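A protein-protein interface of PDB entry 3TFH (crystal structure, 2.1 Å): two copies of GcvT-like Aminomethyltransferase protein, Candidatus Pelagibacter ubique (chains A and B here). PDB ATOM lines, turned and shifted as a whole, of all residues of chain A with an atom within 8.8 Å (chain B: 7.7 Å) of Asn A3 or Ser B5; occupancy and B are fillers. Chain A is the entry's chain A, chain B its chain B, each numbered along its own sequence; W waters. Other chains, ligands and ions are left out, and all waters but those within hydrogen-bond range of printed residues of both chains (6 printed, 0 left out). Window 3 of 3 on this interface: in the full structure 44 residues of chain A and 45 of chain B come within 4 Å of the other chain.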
ATOM      1  N   MET A   1     -17.032  23.669 -16.381  1.00  0.00           N
ATOM      2  CA  MET A   1     -18.201  23.407 -17.245  1.00  0.00           C
ATOM      3  C   MET A   1     -19.121  24.644 -17.302  1.00  0.00           C
ATOM      4  O   MET A   1     -19.135  25.417 -16.354  1.00  0.00           O
ATOM      5  CB  MET A   1     -18.917  22.157 -16.697  1.00  0.00           C
ATOM      6  CG  MET A   1     -18.039  20.887 -16.692  1.00  0.00           C
ATOM      7  SD  MET A   1     -17.814  20.110 -18.341  1.00  0.00           S
ATOM      8  CE  MET A   1     -19.527  19.627 -18.702  1.00  0.00           C
ATOM      9  N   LYS A   2     -19.874  24.852 -18.393  1.00  0.00           N
ATOM     10  CA  LYS A   2     -20.841  25.938 -18.461  1.00  0.00           C
ATOM     11  C   LYS A   2     -22.100  25.581 -17.674  1.00  0.00           C
ATOM     12  O   LYS A   2     -22.628  26.421 -16.982  1.00  0.00           O
ATOM     13  CB  LYS A   2     -21.308  26.283 -19.873  1.00  0.00           C
ATOM     14  CG  LYS A   2     -21.971  27.593 -19.893  1.00  0.00           C
ATOM     15  CD  LYS A   2     -22.737  27.850 -21.104  1.00  0.00           C
ATOM     16  CE  LYS A   2     -23.826  28.883 -20.846  1.00  0.00           C
ATOM     17  NZ  LYS A   2     -23.468  30.275 -21.260  1.00  0.00           N
ATOM     18  N   ASN A   3     -22.562  24.350 -17.838  1.00  0.00           N
ATOM     19  CA  ASN A   3     -23.711  23.819 -17.118  1.00  0.00           C
ATOM     20  C   ASN A   3     -23.294  22.625 -16.288  1.00  0.00           C
ATOM     21  O   ASN A   3     -22.321  21.889 -16.585  1.00  0.00           O
ATOM     22  CB  ASN A   3     -24.848  23.402 -18.074  1.00  0.00           C
ATOM     23  CG  ASN A   3     -25.447  24.578 -18.816  1.00  0.00           C
ATOM     24  OD1 ASN A   3     -25.284  24.692 -20.041  1.00  0.00           O
ATOM     25  ND2 ASN A   3     -26.101  25.478 -18.094  1.00  0.00           N
ATOM     26  N   PHE A   4     -24.021  22.457 -15.208  1.00  0.00           N
ATOM     27  CA  PHE A   4     -23.758  21.412 -14.297  1.00  0.00           C
ATOM     28  C   PHE A   4     -24.964  20.487 -14.338  1.00  0.00           C
ATOM     29  O   PHE A   4     -26.116  20.927 -14.479  1.00  0.00           O
ATOM     30  CB  PHE A   4     -23.488  22.041 -12.919  1.00  0.00           C
ATOM     31  CG  PHE A   4     -22.398  23.096 -12.959  1.00  0.00           C
ATOM     32  CD1 PHE A   4     -21.061  22.726 -12.955  1.00  0.00           C
ATOM     33  CD2 PHE A   4     -22.711  24.461 -13.045  1.00  0.00           C
ATOM     34  CE1 PHE A   4     -20.053  23.676 -13.044  1.00  0.00           C
ATOM     35  CE2 PHE A   4     -21.696  25.424 -13.089  1.00  0.00           C
ATOM     36  CZ  PHE A   4     -20.367  25.026 -13.096  1.00  0.00           C
ATOM     37  N   SER A   5     -24.723  19.210 -14.271  1.00  0.00           N
ATOM     38  CA  SER A   5     -25.823  18.279 -14.254  1.00  0.00           C
ATOM     39  C   SER A   5     -26.478  18.280 -12.863  1.00  0.00           C
ATOM     40  O   SER A   5     -25.846  18.614 -11.839  1.00  0.00           O
ATOM     41  CB  SER A   5     -25.381  16.883 -14.698  1.00  0.00           C
ATOM     42  OG  SER A   5     -24.536  16.266 -13.749  1.00  0.00           O
ATOM     43  N   ILE A   6     -27.746  17.933 -12.842  1.00  0.00           N
ATOM     44  CA  ILE A   6     -28.425  17.701 -11.597  1.00  0.00           C
ATOM     45  C   ILE A   6     -28.185  16.219 -11.249  1.00  0.00           C
ATOM     46  O   ILE A   6     -28.318  15.317 -12.109  1.00  0.00           O
ATOM     47  CB  ILE A   6     -29.915  18.083 -11.689  1.00  0.00           C
ATOM     48  CG1 ILE A   6     -30.544  18.104 -10.279  1.00  0.00           C
ATOM     49  CG2 ILE A   6     -30.614  17.142 -12.612  1.00  0.00           C
ATOM     50  CD1 ILE A   6     -31.720  19.031 -10.212  1.00  0.00           C
ATOM     51  N   ALA A   7     -27.768  15.959 -10.033  1.00  0.00           N
ATOM     52  CA  ALA A   7     -27.570  14.582  -9.543  1.00  0.00           C
ATOM     53  C   ALA A   7     -28.844  14.018  -8.925  1.00  0.00           C
ATOM     54  O   ALA A   7     -29.265  14.417  -7.807  1.00  0.00           O
ATOM     55  CB  ALA A   7     -26.411  14.537  -8.535  1.00  0.00           C
ATOM     56  N   LYS A   8     -29.449  13.047  -9.602  1.00  0.00           N
ATOM     57  CA  LYS A   8     -30.694  12.404  -9.135  1.00  0.00           C
ATOM     58  C   LYS A   8     -30.410  11.457  -7.957  1.00  0.00           C
ATOM     59  O   LYS A   8     -29.326  10.937  -7.836  1.00  0.00           O
ATOM     60  CB  LYS A   8     -31.344  11.646 -10.300  1.00  0.00           C
ATOM     61  CG  LYS A   8     -32.043  12.603 -11.298  1.00  0.00           C
ATOM     62  CD  LYS A   8     -32.816  11.836 -12.306  1.00  0.00           C
ATOM     63  CE  LYS A   8     -33.413  12.739 -13.394  1.00  0.00           C
ATOM     64  NZ  LYS A   8     -34.201  11.842 -14.235  1.00  0.00           N
ATOM     65  N   VAL A  26     -37.681  17.904 -21.786  1.00  0.00           N
ATOM     66  CA  VAL A  26     -37.240  18.780 -20.688  1.00  0.00           C
ATOM     67  C   VAL A  26     -35.724  19.009 -20.830  1.00  0.00           C
ATOM     68  O   VAL A  26     -35.008  18.094 -21.103  1.00  0.00           O
ATOM     69  CB  VAL A  26     -37.612  18.191 -19.289  1.00  0.00           C
ATOM     70  CG1 VAL A  26     -36.793  16.933 -19.020  1.00  0.00           C
ATOM     71  CG2 VAL A  26     -37.396  19.224 -18.189  1.00  0.00           C
ATOM     72  N   THR A  27     -35.230  20.240 -20.698  1.00  0.00           N
ATOM     73  CA  THR A  27     -33.776  20.457 -20.854  1.00  0.00           C
ATOM     74  C   THR A  27     -33.110  20.987 -19.565  1.00  0.00           C
ATOM     75  O   THR A  27     -31.877  21.000 -19.480  1.00  0.00           O
ATOM     76  CB  THR A  27     -33.457  21.476 -21.939  1.00  0.00           C
ATOM     77  OG1 THR A  27     -34.126  22.704 -21.660  1.00  0.00           O
ATOM     78  CG2 THR A  27     -33.848  20.945 -23.342  1.00  0.00           C
ATOM     79  N   ALA A  28     -33.893  21.447 -18.574  1.00  0.00           N
ATOM     80  CA  ALA A  28     -33.309  21.798 -17.305  1.00  0.00           C
ATOM     81  C   ALA A  28     -34.294  21.607 -16.150  1.00  0.00           C
ATOM     82  O   ALA A  28     -35.492  21.611 -16.360  1.00  0.00           O
ATOM     83  CB  ALA A  28     -32.722  23.221 -17.339  1.00  0.00           C
ATOM     84  N   TYR A  29     -33.749  21.353 -14.969  1.00  0.00           N
ATOM     85  CA  TYR A  29     -34.522  21.161 -13.737  1.00  0.00           C
ATOM     86  C   TYR A  29     -34.089  22.148 -12.677  1.00  0.00           C
ATOM     87  O   TYR A  29     -32.910  22.589 -12.603  1.00  0.00           O
ATOM     88  CB  TYR A  29     -34.326  19.767 -13.163  1.00  0.00           C
ATOM     89  CG  TYR A  29     -35.085  18.653 -13.793  1.00  0.00           C
ATOM     90  CD1 TYR A  29     -36.492  18.550 -13.654  1.00  0.00           C
ATOM     91  CD2 TYR A  29     -34.417  17.641 -14.493  1.00  0.00           C
ATOM     92  CE1 TYR A  29     -37.192  17.473 -14.181  1.00  0.00           C
ATOM     93  CE2 TYR A  29     -35.117  16.575 -15.012  1.00  0.00           C
ATOM     94  CZ  TYR A  29     -36.498  16.497 -14.860  1.00  0.00           C
ATOM     95  OH  TYR A  29     -37.179  15.444 -15.368  1.00  0.00           O
ATOM     96  N   THR A  30     -35.086  22.526 -11.876  1.00  0.00           N
ATOM     97  CA  THR A  30     -34.841  23.090 -10.610  1.00  0.00           C
ATOM     98  C   THR A  30     -35.346  22.090  -9.558  1.00  0.00           C
ATOM     99  O   THR A  30     -35.835  21.004  -9.891  1.00  0.00           O
ATOM    100  CB  THR A  30     -35.445  24.496 -10.489  1.00  0.00           C
ATOM    101  OG1 THR A  30     -34.997  25.068  -9.266  1.00  0.00           O
ATOM    102  CG2 THR A  30     -36.993  24.534 -10.612  1.00  0.00           C
ATOM    103  N   ILE A  31     -35.047  22.411  -8.304  1.00  0.00           N
ATOM    104  CA  ILE A  31     -35.452  21.605  -7.208  1.00  0.00           C
ATOM    105  C   ILE A  31     -36.379  22.527  -6.378  1.00  0.00           C
ATOM    106  O   ILE A  31     -36.042  23.677  -6.098  1.00  0.00           O
ATOM    107  CB  ILE A  31     -34.301  21.042  -6.327  1.00  0.00           C
ATOM    108  CG1 ILE A  31     -33.492  19.900  -7.006  1.00  0.00           C
ATOM    109  CG2 ILE A  31     -34.874  20.475  -4.889  1.00  0.00           C
ATOM    110  CD1 ILE A  31     -34.274  18.810  -7.623  1.00  0.00           C
ATOM    111  N   LEU A  36     -37.995  17.255  -8.014  1.00  0.00           N
ATOM    112  CA  LEU A  36     -37.694  17.798  -9.344  1.00  0.00           C
ATOM    113  C   LEU A  36     -38.880  18.584  -9.900  1.00  0.00           C
ATOM    114  O   LEU A  36     -40.034  18.122  -9.863  1.00  0.00           O
ATOM    115  CB  LEU A  36     -37.318  16.685 -10.312  1.00  0.00           C
ATOM    116  CG  LEU A  36     -36.033  15.913 -10.026  1.00  0.00           C
ATOM    117  CD1 LEU A  36     -35.952  14.545 -10.792  1.00  0.00           C
ATOM    118  CD2 LEU A  36     -34.850  16.796 -10.373  1.00  0.00           C
ATOM    119  N   LEU A  37     -38.576  19.791 -10.369  1.00  0.00           N
ATOM    120  CA  LEU A  37     -39.530  20.646 -11.118  1.00  0.00           C
ATOM    121  C   LEU A  37     -38.866  21.108 -12.385  1.00  0.00           C
ATOM    122  O   LEU A  37     -37.752  21.668 -12.325  1.00  0.00           O
ATOM    123  CB  LEU A  37     -39.919  21.862 -10.288  1.00  0.00           C
ATOM    124  CG  LEU A  37     -40.764  22.999 -10.845  1.00  0.00           C
ATOM    125  CD1 LEU A  37     -42.237  22.551 -10.890  1.00  0.00           C
ATOM    126  CD2 LEU A  37     -40.586  24.188  -9.927  1.00  0.00           C
ATOM    127  N   PRO A  38     -39.540  20.944 -13.514  1.00  0.00           N
ATOM    128  CA  PRO A  38     -38.937  21.401 -14.774  1.00  0.00           C
ATOM    129  C   PRO A  38     -38.720  22.887 -14.767  1.00  0.00           C
ATOM    130  O   PRO A  38     -39.592  23.640 -14.269  1.00  0.00           O
ATOM    131  CB  PRO A  38     -39.948  21.004 -15.839  1.00  0.00           C
ATOM    132  CG  PRO A  38     -41.125  20.612 -15.139  1.00  0.00           C
ATOM    133  CD  PRO A  38     -40.866  20.333 -13.721  1.00  0.00           C
ATOM    134  N   ALA A  39     -37.543  23.310 -15.263  1.00  0.00           N
ATOM    135  CA  ALA A  39     -37.236  24.736 -15.410  1.00  0.00           C
ATOM    136  C   ALA A  39     -37.162  25.244 -16.874  1.00  0.00           C
ATOM    137  O   ALA A  39     -37.290  26.443 -17.097  1.00  0.00           O
ATOM    138  CB  ALA A  39     -35.929  25.081 -14.694  1.00  0.00           C
ATOM    139  N   ALA A  40     -36.952  24.344 -17.833  1.00  0.00           N
ATOM    140  CA  ALA A  40     -36.937  24.648 -19.281  1.00  0.00           C
ATOM    141  C   ALA A  40     -37.220  23.427 -20.114  1.00  0.00           C
ATOM    142  O   ALA A  40     -36.840  22.300 -19.736  1.00  0.00           O
ATOM    143  CB  ALA A  40     -35.574  25.368 -19.792  1.00  0.00           C
ATOM    144  N   ASN B   3     -28.495  12.761 -18.876  1.00  0.00           N
ATOM    145  CA  ASN B   3     -28.223  13.854 -17.902  1.00  0.00           C
ATOM    146  C   ASN B   3     -29.002  15.138 -18.209  1.00  0.00           C
ATOM    147  O   ASN B   3     -29.324  15.419 -19.357  1.00  0.00           O
ATOM    148  CB  ASN B   3     -26.721  14.181 -17.819  1.00  0.00           C
ATOM    149  CG  ASN B   3     -25.967  13.211 -16.876  1.00  0.00           C
ATOM    150  OD1 ASN B   3     -26.513  12.768 -15.861  1.00  0.00           O
ATOM    151  ND2 ASN B   3     -24.721  12.884 -17.223  1.00  0.00           N
ATOM    152  N   PHE B   4     -29.356  15.873 -17.156  1.00  0.00           N
ATOM    153  CA  PHE B   4     -30.105  17.112 -17.277  1.00  0.00           C
ATOM    154  C   PHE B   4     -29.405  18.212 -16.536  1.00  0.00           C
ATOM    155  O   PHE B   4     -28.858  17.974 -15.411  1.00  0.00           O
ATOM    156  CB  PHE B   4     -31.550  16.930 -16.793  1.00  0.00           C
ATOM    157  CG  PHE B   4     -32.277  15.915 -17.535  1.00  0.00           C
ATOM    158  CD1 PHE B   4     -32.907  16.233 -18.733  1.00  0.00           C
ATOM    159  CD2 PHE B   4     -32.307  14.605 -17.080  1.00  0.00           C
ATOM    160  CE1 PHE B   4     -33.586  15.255 -19.431  1.00  0.00           C
ATOM    161  CE2 PHE B   4     -32.978  13.626 -17.791  1.00  0.00           C
ATOM    162  CZ  PHE B   4     -33.608  13.962 -18.954  1.00  0.00           C
ATOM    163  N   SER B   5     -29.371  19.403 -17.155  1.00  0.00           N
ATOM    164  CA  SER B   5     -28.799  20.614 -16.518  1.00  0.00           C
ATOM    165  C   SER B   5     -29.599  21.106 -15.305  1.00  0.00           C
ATOM    166  O   SER B   5     -30.811  21.042 -15.277  1.00  0.00           O
ATOM    167  CB  SER B   5     -28.614  21.774 -17.521  1.00  0.00           C
ATOM    168  OG  SER B   5     -27.695  21.344 -18.518  1.00  0.00           O
ATOM    169  N   ILE B   6     -28.903  21.637 -14.322  1.00  0.00           N
ATOM    170  CA  ILE B   6     -29.545  22.359 -13.208  1.00  0.00           C
ATOM    171  C   ILE B   6     -29.714  23.820 -13.612  1.00  0.00           C
ATOM    172  O   ILE B   6     -28.859  24.399 -14.261  1.00  0.00           O
ATOM    173  CB  ILE B   6     -28.706  22.234 -11.857  1.00  0.00           C
ATOM    174  CG1 ILE B   6     -29.545  22.571 -10.607  1.00  0.00           C
ATOM    175  CG2 ILE B   6     -27.446  23.106 -11.938  1.00  0.00           C
ATOM    176  CD1 ILE B   6     -28.729  22.475  -9.269  1.00  0.00           C
ATOM    177  N   ALA B   7     -30.839  24.417 -13.265  1.00  0.00           N
ATOM    178  CA  ALA B   7     -31.083  25.810 -13.482  1.00  0.00           C
ATOM    179  C   ALA B   7     -30.811  26.572 -12.183  1.00  0.00           C
ATOM    180  O   ALA B   7     -31.487  26.353 -11.173  1.00  0.00           O
ATOM    181  CB  ALA B   7     -32.573  26.038 -13.994  1.00  0.00           C
ATOM    182  N   LYS B   8     -29.835  27.480 -12.204  1.00  0.00           N
ATOM    183  CA  LYS B   8     -29.475  28.291 -11.024  1.00  0.00           C
ATOM    184  C   LYS B   8     -30.413  29.443 -10.902  1.00  0.00           C
ATOM    185  O   LYS B   8     -30.919  29.934 -11.892  1.00  0.00           O
ATOM    186  CB  LYS B   8     -28.054  28.826 -11.120  1.00  0.00           C
ATOM    187  CG  LYS B   8     -27.069  27.659 -11.037  1.00  0.00           C
ATOM    188  CD  LYS B   8     -25.781  28.164 -10.599  1.00  0.00           C
ATOM    189  CE  LYS B   8     -24.740  27.129 -10.526  1.00  0.00           C
ATOM    190  NZ  LYS B   8     -23.517  27.945 -10.581  1.00  0.00           N
ATOM    191  N   VAL B  26     -15.970  21.016 -10.692  1.00  0.00           N
ATOM    192  CA  VAL B  26     -17.290  20.465 -10.304  1.00  0.00           C
ATOM    193  C   VAL B  26     -18.104  20.211 -11.592  1.00  0.00           C
ATOM    194  O   VAL B  26     -18.161  21.060 -12.486  1.00  0.00           O
ATOM    195  CB  VAL B  26     -18.030  21.364  -9.276  1.00  0.00           C
ATOM    196  CG1 VAL B  26     -18.542  22.686  -9.887  1.00  0.00           C
ATOM    197  CG2 VAL B  26     -19.162  20.603  -8.549  1.00  0.00           C
ATOM    198  N   THR B  27     -18.711  19.022 -11.687  1.00  0.00           N
ATOM    199  CA  THR B  27     -19.509  18.667 -12.853  1.00  0.00           C
ATOM    200  C   THR B  27     -21.012  18.500 -12.553  1.00  0.00           C
ATOM    201  O   THR B  27     -21.851  18.585 -13.455  1.00  0.00           O
ATOM    202  CB  THR B  27     -18.955  17.396 -13.467  1.00  0.00           C
ATOM    203  OG1 THR B  27     -18.894  16.388 -12.466  1.00  0.00           O
ATOM    204  CG2 THR B  27     -17.465  17.624 -14.120  1.00  0.00           C
ATOM    205  N   ALA B  28     -21.364  18.218 -11.302  1.00  0.00           N
ATOM    206  CA  ALA B  28     -22.730  17.927 -10.925  1.00  0.00           C
ATOM    207  C   ALA B  28     -23.038  18.483  -9.541  1.00  0.00           C
ATOM    208  O   ALA B  28     -22.162  18.486  -8.692  1.00  0.00           O
ATOM    209  CB  ALA B  28     -23.055  16.377 -10.968  1.00  0.00           C
ATOM    210  N   TYR B  29     -24.290  18.923  -9.354  1.00  0.00           N
ATOM    211  CA  TYR B  29     -24.821  19.403  -8.105  1.00  0.00           C
ATOM    212  C   TYR B  29     -26.060  18.680  -7.660  1.00  0.00           C
ATOM    213  O   TYR B  29     -26.874  18.243  -8.473  1.00  0.00           O
ATOM    214  CB  TYR B  29     -25.246  20.896  -8.167  1.00  0.00           C
ATOM    215  CG  TYR B  29     -24.122  21.910  -8.153  1.00  0.00           C
ATOM    216  CD1 TYR B  29     -23.427  22.161  -7.022  1.00  0.00           C
ATOM    217  CD2 TYR B  29     -23.818  22.655  -9.276  1.00  0.00           C
ATOM    218  CE1 TYR B  29     -22.428  23.122  -6.975  1.00  0.00           C
ATOM    219  CE2 TYR B  29     -22.812  23.607  -9.271  1.00  0.00           C
ATOM    220  CZ  TYR B  29     -22.101  23.844  -8.124  1.00  0.00           C
ATOM    221  OH  TYR B  29     -21.156  24.854  -8.052  1.00  0.00           O
HETATM  222  O   HOH W   1     -20.954  19.476 -16.121  1.00  0.00           O
HETATM  223  O   HOH W   2     -30.050  19.024 -20.340  1.00  0.00           O
HETATM  224  O   HOH W   3     -16.524  23.068 -13.529  1.00  0.00           O
HETATM  225  O   HOH W   4     -33.743  27.325 -10.036  1.00  0.00           O
HETATM  226  O   HOH W   5     -26.205  24.292 -14.952  1.00  0.00           O
HETATM  227  O   HOH W   6     -29.342  14.570 -14.456  1.00  0.00           O
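Of the 10 printed residues of chain B, 9 touch a printed residue of chain A.
Of the 19 printed residues of chain A, 10 touch a printed residue of chain B.
Hydrophobic or aromatic side chains of chain A within 4 Å of the printed part of chain B: Phe A4, Ile A6, Ala A7, Val A26, Ala A28, Tyr A29 and Ala A39.
Among the printed residues, 22 pairs touch across the chains.
Among the printed residues, no Asp or Glu carboxylate lies within 4 Å of a Lys or Arg side-chain nitrogen of the other chain.
Water W6 bridges O of Ile A6 (2.7 Å) and N of Phe B4 (3.0 Å).
Water W4 bridges the side-chain hydroxyl of Thr A30 (2.7 Å) and the backbone carbonyl oxygen of Ala B7 (2.7 Å).
Water W5 lies within hydrogen-bond range of the backbone carbonyl oxygen (O) of Ile B6 (2.7 Å), the backbone NH (N) of Phe A4 (2.9 Å) and the side-chain amide nitrogen (ND2) of Asn A3 (3.4 Å).
Water W3 lies within hydrogen-bond range of the backbone carbonyl oxygen of Val B26 (2.8 Å) and the backbone NH of Met A1 (3.0 Å).
Water W1 bridges the backbone carbonyl oxygen of Asn A3 (2.8 Å) and the backbone carbonyl oxygen of Thr B27 (3.0 Å).
Water W2 lies within hydrogen-bond range of O of Thr A27 (2.8 Å) and N of Ser B5 (3.3 Å).
Among the printed residues, pairs that only touch across the chains: Ser A5 with Ala B28 (3.2 Å), Ser A5 with Phe B4 (3.3 Å), Phe A4 with Val B26 (3.3 Å), Ala A28 with Ser B5 (3.3 Å), Phe A4 with Ser B5 (3.4 Å), Tyr A29 with Ile B6 (3.4 Å), Phe A4 with Thr B27 (3.5 Å), Ile A6 with Tyr B29 (3.5 Å), Asn A3 with Ser B5 (3.5 Å), Ala A39 with Ala B7 (3.6 Å), Val A26 with Phe B4 (3.6 Å), Phe A4 with Tyr B29 (3.7 Å), Tyr A29 with Phe B4 (3.7 Å), Thr A27 with Ser B5 (3.8 Å) and Phe A4 with Lys B8 (3.995 Å).
Lys A2 touches none of the printed residues of chain B.
Printed residues of chain B within 4 Å of Ser A5: Phe B4, Thr B27, Ala B28 and Tyr B29.
Of the printed residues of chain B, Thr A27 touches Ser B5 (3.8 Å).
Ser B5 touches five residues of chain A.
Printed residues of chain A within 4 Å of Ile B6: Phe A4 (2.9 Å) and Tyr A29 (3.4 Å).
Printed residues of chain A within 4 Å of Thr B27: Phe A4 (3.5 Å) and Ser A5 (3.1 Å).
Of the printed residues of chain A, Ala B28 touches Ser A5 (3.2 Å).
The nearest printed residue of chain B that does not touch Ser A5 is Asn B3 (4.3 Å).
The backbone NH (N) of Ile B6 is in hydrogen-bond range of the backbone carbonyl oxygen (O) of Phe A4 (2.9 Å).
O of Ser B5 is in hydrogen-bond range of N of Tyr A29 (3.0 Å).
O of Phe B4 sits at hydrogen-bond distance from N of Ile A6 (2.8 Å).
O of Thr B27 lies within hydrogen-bond range of N of Ser A5 (3.1 Å).
O of Ser A5 sits at hydrogen-bond distance from N of Tyr B29 (2.9 Å).
The backbone carbonyl oxygen (O) of Tyr A29 lies within hydrogen-bond range of the backbone NH (N) of Ala B7, at 2.8 Å.
The backbone carbonyl oxygen (O) of Tyr B29 lies within hydrogen-bond range of the backbone NH (N) of Ala A7 (2.9 Å).
Phe A4 touches Lys B8, but with the chains exchanged Lys A8 does not touch Phe B4 (4.2 Å).
Phe A4 touches Val B26, and with the chains exchanged Val A26 touches Phe B4.
Phe A4 touches Tyr B29, and with the chains exchanged Tyr A29 touches Phe B4.
Ile A6 touches Tyr B29, and with the chains exchanged Tyr A29 touches Ile B6.
Positions printed for both chains: 3, 4, 5, 6, 7, 8, 26, 27, 28 and 29.
Of the 22 pairs that touch across the chains among the printed residues, 18 have their exchanged pair printed and touching as well.
The backbone NH of Ala A28 lies within hydrogen-bond range of the backbone carbonyl oxygen of Ala A40, at 3.3 Å.
The backbone carbonyl oxygen (O) of Ala A40 sits at hydrogen-bond distance from the backbone NH (N) of Thr A27, at 2.8 Å.
The backbone carbonyl oxygen of Ala A28 is in hydrogen-bond range of the backbone NH of Ala A39, at 2.9 Å.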
